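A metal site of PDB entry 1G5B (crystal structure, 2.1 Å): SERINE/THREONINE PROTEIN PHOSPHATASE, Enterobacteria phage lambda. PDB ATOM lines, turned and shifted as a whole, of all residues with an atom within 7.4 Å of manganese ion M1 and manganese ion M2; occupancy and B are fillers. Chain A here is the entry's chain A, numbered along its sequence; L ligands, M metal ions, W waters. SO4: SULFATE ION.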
ATOM      1  N   GLY A  19     -33.160   1.733  32.338  1.00  0.00           N
ATOM      2  CA  GLY A  19     -32.908   2.189  30.974  1.00  0.00           C
ATOM      3  C   GLY A  19     -31.991   3.403  30.929  1.00  0.00           C
ATOM      4  O   GLY A  19     -31.462   3.837  31.950  1.00  0.00           O
ATOM      5  N   ASP A  20     -31.797   3.958  29.729  1.00  0.00           N
ATOM      6  CA  ASP A  20     -30.924   5.118  29.522  1.00  0.00           C
ATOM      7  C   ASP A  20     -31.151   6.222  30.545  1.00  0.00           C
ATOM      8  O   ASP A  20     -32.279   6.692  30.715  1.00  0.00           O
ATOM      9  CB  ASP A  20     -31.131   5.651  28.094  1.00  0.00           C
ATOM     10  CG  ASP A  20     -30.897   4.589  27.041  1.00  0.00           C
ATOM     11  OD1 ASP A  20     -31.440   3.481  27.211  1.00  0.00           O
ATOM     12  OD2 ASP A  20     -30.182   4.851  26.043  1.00  0.00           O
ATOM     13  N   LEU A  21     -30.084   6.618  31.221  1.00  0.00           N
ATOM     14  CA  LEU A  21     -30.175   7.657  32.252  1.00  0.00           C
ATOM     15  C   LEU A  21     -29.944   9.093  31.782  1.00  0.00           C
ATOM     16  O   LEU A  21     -30.626  10.007  32.254  1.00  0.00           O
ATOM     17  CB  LEU A  21     -29.193   7.332  33.381  1.00  0.00           C
ATOM     18  CG  LEU A  21     -29.664   6.180  34.278  1.00  0.00           C
ATOM     19  CD1 LEU A  21     -28.536   5.729  35.197  1.00  0.00           C
ATOM     20  CD2 LEU A  21     -30.878   6.655  35.088  1.00  0.00           C
ATOM     21  N   HIS A  22     -28.981   9.288  30.889  1.00  0.00           N
ATOM     22  CA  HIS A  22     -28.670  10.611  30.362  1.00  0.00           C
ATOM     23  C   HIS A  22     -28.784  11.734  31.389  1.00  0.00           C
ATOM     24  O   HIS A  22     -29.594  12.646  31.239  1.00  0.00           O
ATOM     25  CB  HIS A  22     -29.564  10.933  29.166  1.00  0.00           C
ATOM     26  CG  HIS A  22     -29.315  10.067  27.973  1.00  0.00           C
ATOM     27  ND1 HIS A  22     -28.101  10.024  27.325  1.00  0.00           N
ATOM     28  CD2 HIS A  22     -30.120   9.198  27.310  1.00  0.00           C
ATOM     29  CE1 HIS A  22     -28.167   9.171  26.317  1.00  0.00           C
ATOM     30  NE2 HIS A  22     -29.379   8.652  26.297  1.00  0.00           N
ATOM     31  N   VAL A  47     -28.122  -0.232  31.377  1.00  0.00           N
ATOM     32  CA  VAL A  47     -27.913  -0.485  29.950  1.00  0.00           C
ATOM     33  C   VAL A  47     -26.964   0.527  29.319  1.00  0.00           C
ATOM     34  O   VAL A  47     -26.695   0.474  28.121  1.00  0.00           O
ATOM     35  CB  VAL A  47     -29.253  -0.444  29.170  1.00  0.00           C
ATOM     36  CG1 VAL A  47     -30.222  -1.464  29.729  1.00  0.00           C
ATOM     37  CG2 VAL A  47     -29.848   0.966  29.225  1.00  0.00           C
ATOM     38  N   GLY A  48     -26.452   1.460  30.110  1.00  0.00           N
ATOM     39  CA  GLY A  48     -25.550   2.445  29.563  1.00  0.00           C
ATOM     40  C   GLY A  48     -26.211   3.759  29.200  1.00  0.00           C
ATOM     41  O   GLY A  48     -27.399   3.966  29.490  1.00  0.00           O
ATOM     42  N   ASP A  49     -25.456   4.645  28.537  1.00  0.00           N
ATOM     43  CA  ASP A  49     -25.931   5.972  28.161  1.00  0.00           C
ATOM     44  C   ASP A  49     -26.264   6.735  29.425  1.00  0.00           C
ATOM     45  O   ASP A  49     -27.384   7.203  29.652  1.00  0.00           O
ATOM     46  CB  ASP A  49     -27.161   5.880  27.234  1.00  0.00           C
ATOM     47  CG  ASP A  49     -26.782   5.911  25.762  1.00  0.00           C
ATOM     48  OD1 ASP A  49     -25.577   5.719  25.451  1.00  0.00           O
ATOM     49  OD2 ASP A  49     -27.666   6.107  24.918  1.00  0.00           O
ATOM     50  N   LEU A  50     -25.247   6.844  30.271  1.00  0.00           N
ATOM     51  CA  LEU A  50     -25.346   7.521  31.561  1.00  0.00           C
ATOM     52  C   LEU A  50     -25.241   9.040  31.423  1.00  0.00           C
ATOM     53  O   LEU A  50     -25.764   9.774  32.269  1.00  0.00           O
ATOM     54  CB  LEU A  50     -24.215   7.047  32.475  1.00  0.00           C
ATOM     55  CG  LEU A  50     -24.013   5.530  32.662  1.00  0.00           C
ATOM     56  CD1 LEU A  50     -22.785   5.282  33.508  1.00  0.00           C
ATOM     57  CD2 LEU A  50     -25.242   4.923  33.324  1.00  0.00           C
ATOM     58  N   VAL A  51     -24.589   9.497  30.366  1.00  0.00           N
ATOM     59  CA  VAL A  51     -24.383  10.932  30.164  1.00  0.00           C
ATOM     60  C   VAL A  51     -24.921  11.513  28.862  1.00  0.00           C
ATOM     61  O   VAL A  51     -25.403  10.793  27.980  1.00  0.00           O
ATOM     62  CB  VAL A  51     -22.895  11.254  30.266  1.00  0.00           C
ATOM     63  CG1 VAL A  51     -22.361  10.879  31.639  1.00  0.00           C
ATOM     64  CG2 VAL A  51     -22.119  10.505  29.184  1.00  0.00           C
ATOM     65  N   ASP A  52     -24.814  12.836  28.758  1.00  0.00           N
ATOM     66  CA  ASP A  52     -25.242  13.620  27.595  1.00  0.00           C
ATOM     67  C   ASP A  52     -26.719  14.011  27.576  1.00  0.00           C
ATOM     68  O   ASP A  52     -27.575  13.257  28.040  1.00  0.00           O
ATOM     69  CB  ASP A  52     -24.919  12.883  26.295  1.00  0.00           C
ATOM     70  CG  ASP A  52     -23.428  12.671  26.089  1.00  0.00           C
ATOM     71  OD1 ASP A  52     -22.616  13.304  26.796  1.00  0.00           O
ATOM     72  OD2 ASP A  52     -23.073  11.877  25.196  1.00  0.00           O
ATOM     73  N   GLY A  74     -22.582   2.437  26.898  1.00  0.00           N
ATOM     74  CA  GLY A  74     -23.519   2.778  25.842  1.00  0.00           C
ATOM     75  C   GLY A  74     -22.771   3.523  24.744  1.00  0.00           C
ATOM     76  O   GLY A  74     -21.585   3.814  24.912  1.00  0.00           O
ATOM     77  N   ASN A  75     -23.427   3.835  23.629  1.00  0.00           N
ATOM     78  CA  ASN A  75     -22.723   4.552  22.573  1.00  0.00           C
ATOM     79  C   ASN A  75     -22.307   5.959  23.025  1.00  0.00           C
ATOM     80  O   ASN A  75     -21.336   6.527  22.523  1.00  0.00           O
ATOM     81  CB  ASN A  75     -23.545   4.589  21.262  1.00  0.00           C
ATOM     82  CG  ASN A  75     -24.891   5.296  21.380  1.00  0.00           C
ATOM     83  OD1 ASN A  75     -25.719   4.968  22.234  1.00  0.00           O
ATOM     84  ND2 ASN A  75     -25.126   6.271  20.502  1.00  0.00           N
ATOM     85  N   HIS A  76     -23.011   6.514  24.018  1.00  0.00           N
ATOM     86  CA  HIS A  76     -22.642   7.826  24.506  1.00  0.00           C
ATOM     87  C   HIS A  76     -21.355   7.737  25.322  1.00  0.00           C
ATOM     88  O   HIS A  76     -20.511   8.631  25.242  1.00  0.00           O
ATOM     89  CB  HIS A  76     -23.798   8.431  25.315  1.00  0.00           C
ATOM     90  CG  HIS A  76     -24.861   9.039  24.450  1.00  0.00           C
ATOM     91  ND1 HIS A  76     -24.972  10.394  24.237  1.00  0.00           N
ATOM     92  CD2 HIS A  76     -25.821   8.459  23.678  1.00  0.00           C
ATOM     93  CE1 HIS A  76     -25.928  10.624  23.368  1.00  0.00           C
ATOM     94  NE2 HIS A  76     -26.461   9.465  23.009  1.00  0.00           N
ATOM     95  N   GLU A  77     -21.190   6.673  26.108  1.00  0.00           N
ATOM     96  CA  GLU A  77     -19.950   6.533  26.873  1.00  0.00           C
ATOM     97  C   GLU A  77     -18.797   6.416  25.870  1.00  0.00           C
ATOM     98  O   GLU A  77     -17.727   7.006  26.052  1.00  0.00           O
ATOM     99  CB  GLU A  77     -19.966   5.282  27.757  1.00  0.00           C
ATOM    100  CG  GLU A  77     -20.653   5.468  29.095  1.00  0.00           C
ATOM    101  CD  GLU A  77     -22.159   5.619  28.977  1.00  0.00           C
ATOM    102  OE1 GLU A  77     -22.726   6.451  29.711  1.00  0.00           O
ATOM    103  OE2 GLU A  77     -22.765   4.893  28.168  1.00  0.00           O
ATOM    104  N   MET A  79     -18.627   7.617  22.785  1.00  0.00           N
ATOM    105  CA  MET A  79     -18.353   8.906  22.131  1.00  0.00           C
ATOM    106  C   MET A  79     -17.579   9.821  23.075  1.00  0.00           C
ATOM    107  O   MET A  79     -16.696  10.566  22.641  1.00  0.00           O
ATOM    108  CB  MET A  79     -19.655   9.595  21.692  1.00  0.00           C
ATOM    109  CG  MET A  79     -20.329   8.917  20.496  1.00  0.00           C
ATOM    110  SD  MET A  79     -21.723   9.876  19.846  1.00  0.00           S
ATOM    111  CE  MET A  79     -23.073   9.153  20.776  1.00  0.00           C
ATOM    112  N   HIS A 139     -26.391  -2.473  25.442  1.00  0.00           N
ATOM    113  CA  HIS A 139     -27.004  -1.174  25.267  1.00  0.00           C
ATOM    114  C   HIS A 139     -28.023  -1.129  24.125  1.00  0.00           C
ATOM    115  O   HIS A 139     -29.172  -0.741  24.325  1.00  0.00           O
ATOM    116  CB  HIS A 139     -25.962  -0.084  25.020  1.00  0.00           C
ATOM    117  CG  HIS A 139     -26.563   1.270  24.800  1.00  0.00           C
ATOM    118  ND1 HIS A 139     -27.336   1.895  25.759  1.00  0.00           N
ATOM    119  CD2 HIS A 139     -26.598   2.062  23.710  1.00  0.00           C
ATOM    120  CE1 HIS A 139     -27.824   3.022  25.269  1.00  0.00           C
ATOM    121  NE2 HIS A 139     -27.392   3.143  24.023  1.00  0.00           N
ATOM    122  N   ALA A 140     -27.613  -1.527  22.923  1.00  0.00           N
ATOM    123  CA  ALA A 140     -28.517  -1.487  21.779  1.00  0.00           C
ATOM    124  C   ALA A 140     -28.978  -2.848  21.281  1.00  0.00           C
ATOM    125  O   ALA A 140     -30.155  -3.024  20.954  1.00  0.00           O
ATOM    126  CB  ALA A 140     -27.862  -0.716  20.612  1.00  0.00           C
ATOM    127  N   ILE A 159     -23.633  -1.412  20.517  1.00  0.00           N
ATOM    128  CA  ILE A 159     -24.076  -0.124  21.050  1.00  0.00           C
ATOM    129  C   ILE A 159     -24.777   0.847  20.103  1.00  0.00           C
ATOM    130  O   ILE A 159     -25.317   1.859  20.563  1.00  0.00           O
ATOM    131  CB  ILE A 159     -22.890   0.620  21.720  1.00  0.00           C
ATOM    132  CG1 ILE A 159     -21.832   0.966  20.677  1.00  0.00           C
ATOM    133  CG2 ILE A 159     -22.293  -0.265  22.816  1.00  0.00           C
ATOM    134  CD1 ILE A 159     -20.659   1.751  21.252  1.00  0.00           C
ATOM    135  N   TRP A 160     -24.789   0.564  18.802  1.00  0.00           N
ATOM    136  CA  TRP A 160     -25.465   1.459  17.851  1.00  0.00           C
ATOM    137  C   TRP A 160     -26.627   0.847  17.072  1.00  0.00           C
ATOM    138  O   TRP A 160     -27.615   1.513  16.774  1.00  0.00           O
ATOM    139  CB  TRP A 160     -24.480   2.043  16.825  1.00  0.00           C
ATOM    140  CG  TRP A 160     -23.622   3.153  17.334  1.00  0.00           C
ATOM    141  CD1 TRP A 160     -22.356   3.044  17.831  1.00  0.00           C
ATOM    142  CD2 TRP A 160     -23.943   4.553  17.373  1.00  0.00           C
ATOM    143  NE1 TRP A 160     -21.876   4.290  18.177  1.00  0.00           N
ATOM    144  CE2 TRP A 160     -22.831   5.224  17.908  1.00  0.00           C
ATOM    145  CE3 TRP A 160     -25.080   5.295  17.003  1.00  0.00           C
ATOM    146  CZ2 TRP A 160     -22.809   6.620  18.089  1.00  0.00           C
ATOM    147  CZ3 TRP A 160     -25.063   6.678  17.184  1.00  0.00           C
ATOM    148  CH2 TRP A 160     -23.928   7.326  17.720  1.00  0.00           C
ATOM    149  N   ARG A 162     -29.851  -0.628  15.434  1.00  0.00           N
ATOM    150  CA  ARG A 162     -31.290  -0.502  15.681  1.00  0.00           C
ATOM    151  C   ARG A 162     -32.038  -1.383  14.680  1.00  0.00           C
ATOM    152  O   ARG A 162     -33.261  -1.357  14.613  1.00  0.00           O
ATOM    153  CB  ARG A 162     -31.743   0.942  15.514  1.00  0.00           C
ATOM    154  CG  ARG A 162     -31.357   1.875  16.646  1.00  0.00           C
ATOM    155  CD  ARG A 162     -32.219   3.126  16.611  1.00  0.00           C
ATOM    156  NE  ARG A 162     -32.085   3.934  17.814  1.00  0.00           N
ATOM    157  CZ  ARG A 162     -31.155   4.869  18.000  1.00  0.00           C
ATOM    158  NH1 ARG A 162     -30.265   5.120  17.044  1.00  0.00           N
ATOM    159  NH2 ARG A 162     -31.118   5.546  19.133  1.00  0.00           N
ATOM    160  N   GLY A 185     -31.565  -0.913  25.795  1.00  0.00           N
ATOM    161  CA  GLY A 185     -32.045   0.449  25.949  1.00  0.00           C
ATOM    162  C   GLY A 185     -31.799   1.064  24.586  1.00  0.00           C
ATOM    163  O   GLY A 185     -32.210   0.490  23.582  1.00  0.00           O
ATOM    164  N   HIS A 186     -31.147   2.226  24.546  1.00  0.00           N
ATOM    165  CA  HIS A 186     -30.782   2.891  23.300  1.00  0.00           C
ATOM    166  C   HIS A 186     -31.914   3.456  22.426  1.00  0.00           C
ATOM    167  O   HIS A 186     -31.861   4.620  22.036  1.00  0.00           O
ATOM    168  CB  HIS A 186     -29.931   1.945  22.447  1.00  0.00           C
ATOM    169  CG  HIS A 186     -29.331   2.585  21.226  1.00  0.00           C
ATOM    170  ND1 HIS A 186     -28.512   3.694  21.288  1.00  0.00           N
ATOM    171  CD2 HIS A 186     -29.397   2.239  19.918  1.00  0.00           C
ATOM    172  CE1 HIS A 186     -28.101   3.996  20.070  1.00  0.00           C
ATOM    173  NE2 HIS A 186     -28.619   3.124  19.220  1.00  0.00           N
ATOM    174  N   THR A 187     -32.926   2.655  22.120  1.00  0.00           N
ATOM    175  CA  THR A 187     -34.038   3.109  21.293  1.00  0.00           C
ATOM    176  C   THR A 187     -35.249   3.448  22.137  1.00  0.00           C
ATOM    177  O   THR A 187     -35.923   2.560  22.662  1.00  0.00           O
ATOM    178  CB  THR A 187     -34.415   2.038  20.251  1.00  0.00           C
ATOM    179  OG1 THR A 187     -33.285   1.767  19.408  1.00  0.00           O
ATOM    180  CG2 THR A 187     -35.569   2.514  19.386  1.00  0.00           C
ATOM    181  N   PRO A 188     -35.549   4.751  22.293  1.00  0.00           N
ATOM    182  CA  PRO A 188     -36.679   5.248  23.086  1.00  0.00           C
ATOM    183  C   PRO A 188     -38.042   4.798  22.583  1.00  0.00           C
ATOM    184  O   PRO A 188     -38.244   4.565  21.392  1.00  0.00           O
ATOM    185  CB  PRO A 188     -36.524   6.764  22.992  1.00  0.00           C
ATOM    186  CG  PRO A 188     -35.069   6.963  22.679  1.00  0.00           C
ATOM    187  CD  PRO A 188     -34.808   5.870  21.692  1.00  0.00           C
ATOM    188  N   ASP A 202     -35.876   1.700  27.374  1.00  0.00           N
ATOM    189  CA  ASP A 202     -35.538   3.103  27.263  1.00  0.00           C
ATOM    190  C   ASP A 202     -36.827   3.881  26.991  1.00  0.00           C
ATOM    191  O   ASP A 202     -37.309   3.909  25.858  1.00  0.00           O
ATOM    192  CB  ASP A 202     -34.545   3.344  26.129  1.00  0.00           C
ATOM    193  CG  ASP A 202     -34.187   4.822  25.967  1.00  0.00           C
ATOM    194  OD1 ASP A 202     -34.581   5.622  26.837  1.00  0.00           O
ATOM    195  OD2 ASP A 202     -33.504   5.171  24.979  1.00  0.00           O
ATOM    196  N   VAL A 206     -34.699  11.400  29.854  1.00  0.00           N
ATOM    197  CA  VAL A 206     -34.145  12.737  29.656  1.00  0.00           C
ATOM    198  C   VAL A 206     -35.132  13.659  28.932  1.00  0.00           C
ATOM    199  O   VAL A 206     -35.153  14.862  29.174  1.00  0.00           O
ATOM    200  CB  VAL A 206     -32.813  12.671  28.850  1.00  0.00           C
ATOM    201  CG1 VAL A 206     -33.089  12.257  27.415  1.00  0.00           C
ATOM    202  CG2 VAL A 206     -32.121  14.014  28.891  1.00  0.00           C
HETATM  203  S   SO4 L   1     -28.385   7.725  20.599  1.00  0.00           S
HETATM  204  O1  SO4 L   1     -29.786   7.263  20.711  1.00  0.00           O
HETATM  205  O2  SO4 L   1     -27.897   7.484  19.233  1.00  0.00           O
HETATM  206  O3  SO4 L   1     -27.549   6.976  21.559  1.00  0.00           O
HETATM  207  O4  SO4 L   1     -28.308   9.171  20.887  1.00  0.00           O
HETATM  208 MN    MN M   1     -29.733   6.935  24.966  1.00  0.00          MN
HETATM  209 MN    MN M   2     -27.711   4.988  22.900  1.00  0.00          MN
HETATM  210  O   HOH W   1     -29.824   8.934  23.231  1.00  0.00           O
HETATM  211  O   HOH W   2     -29.752   6.019  23.069  1.00  0.00           O
HETATM  212  O   HOH W   3     -31.978   7.326  24.766  1.00  0.00           O
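Manganese ion M2 is bound by OD1 of Asn 75 (2.1 Å), NE2 of His 139 (2.2 Å), ND1 of His 186 (2.2 Å), water W2 (2.3 Å), OD2 of Asp 49 (2.3 Å) and O3 of the ligand (2.4 Å).
Within 4 Å of manganese ion M2: Asp 49, Asn 75, His 139 and His 186. The nearest printed residue that does not touch manganese ion M2 is Asp 20 (4.0004 Å).
The backbone carbonyl oxygen of Trp 160 lies within hydrogen-bond range of a ring nitrogen (NE2) of His 186 (3.1 Å). The backbone NH (N) of Gly 185 lies within hydrogen-bond range of the backbone carbonyl oxygen (O) of His 139. The backbone NH (N) of Asp 49 lies within hydrogen-bond range of the side-chain carboxylate (OE2) of Glu 77 (2.7 Å). O of His 186 lies within hydrogen-bond range of NH2 of Arg 162, 3.1 Å away. The backbone carbonyl oxygen of Asp 49 is in hydrogen-bond range of the backbone NH of Leu 21. N of His 186 sits at hydrogen-bond distance from OD1 of Asp 20 (3.0 Å). O of Asp 52 lies close to ND1 of His 22 (3.4 Å). A ring nitrogen (ND1) of His 22 sits at hydrogen-bond distance from the backbone carbonyl oxygen (O) of Val 51 (2.9 Å).
Within 4 Å of manganese ion M1: Asp 20, His 22 and Asp 49. The nearest printed residue that does not touch manganese ion M1 is Asp 202 (4.2 Å).
Manganese ion M1 is bound by water W2, NE2 of His 22, OD2 of Asp 49, water W3, OD2 of Asp 20 and water W1.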
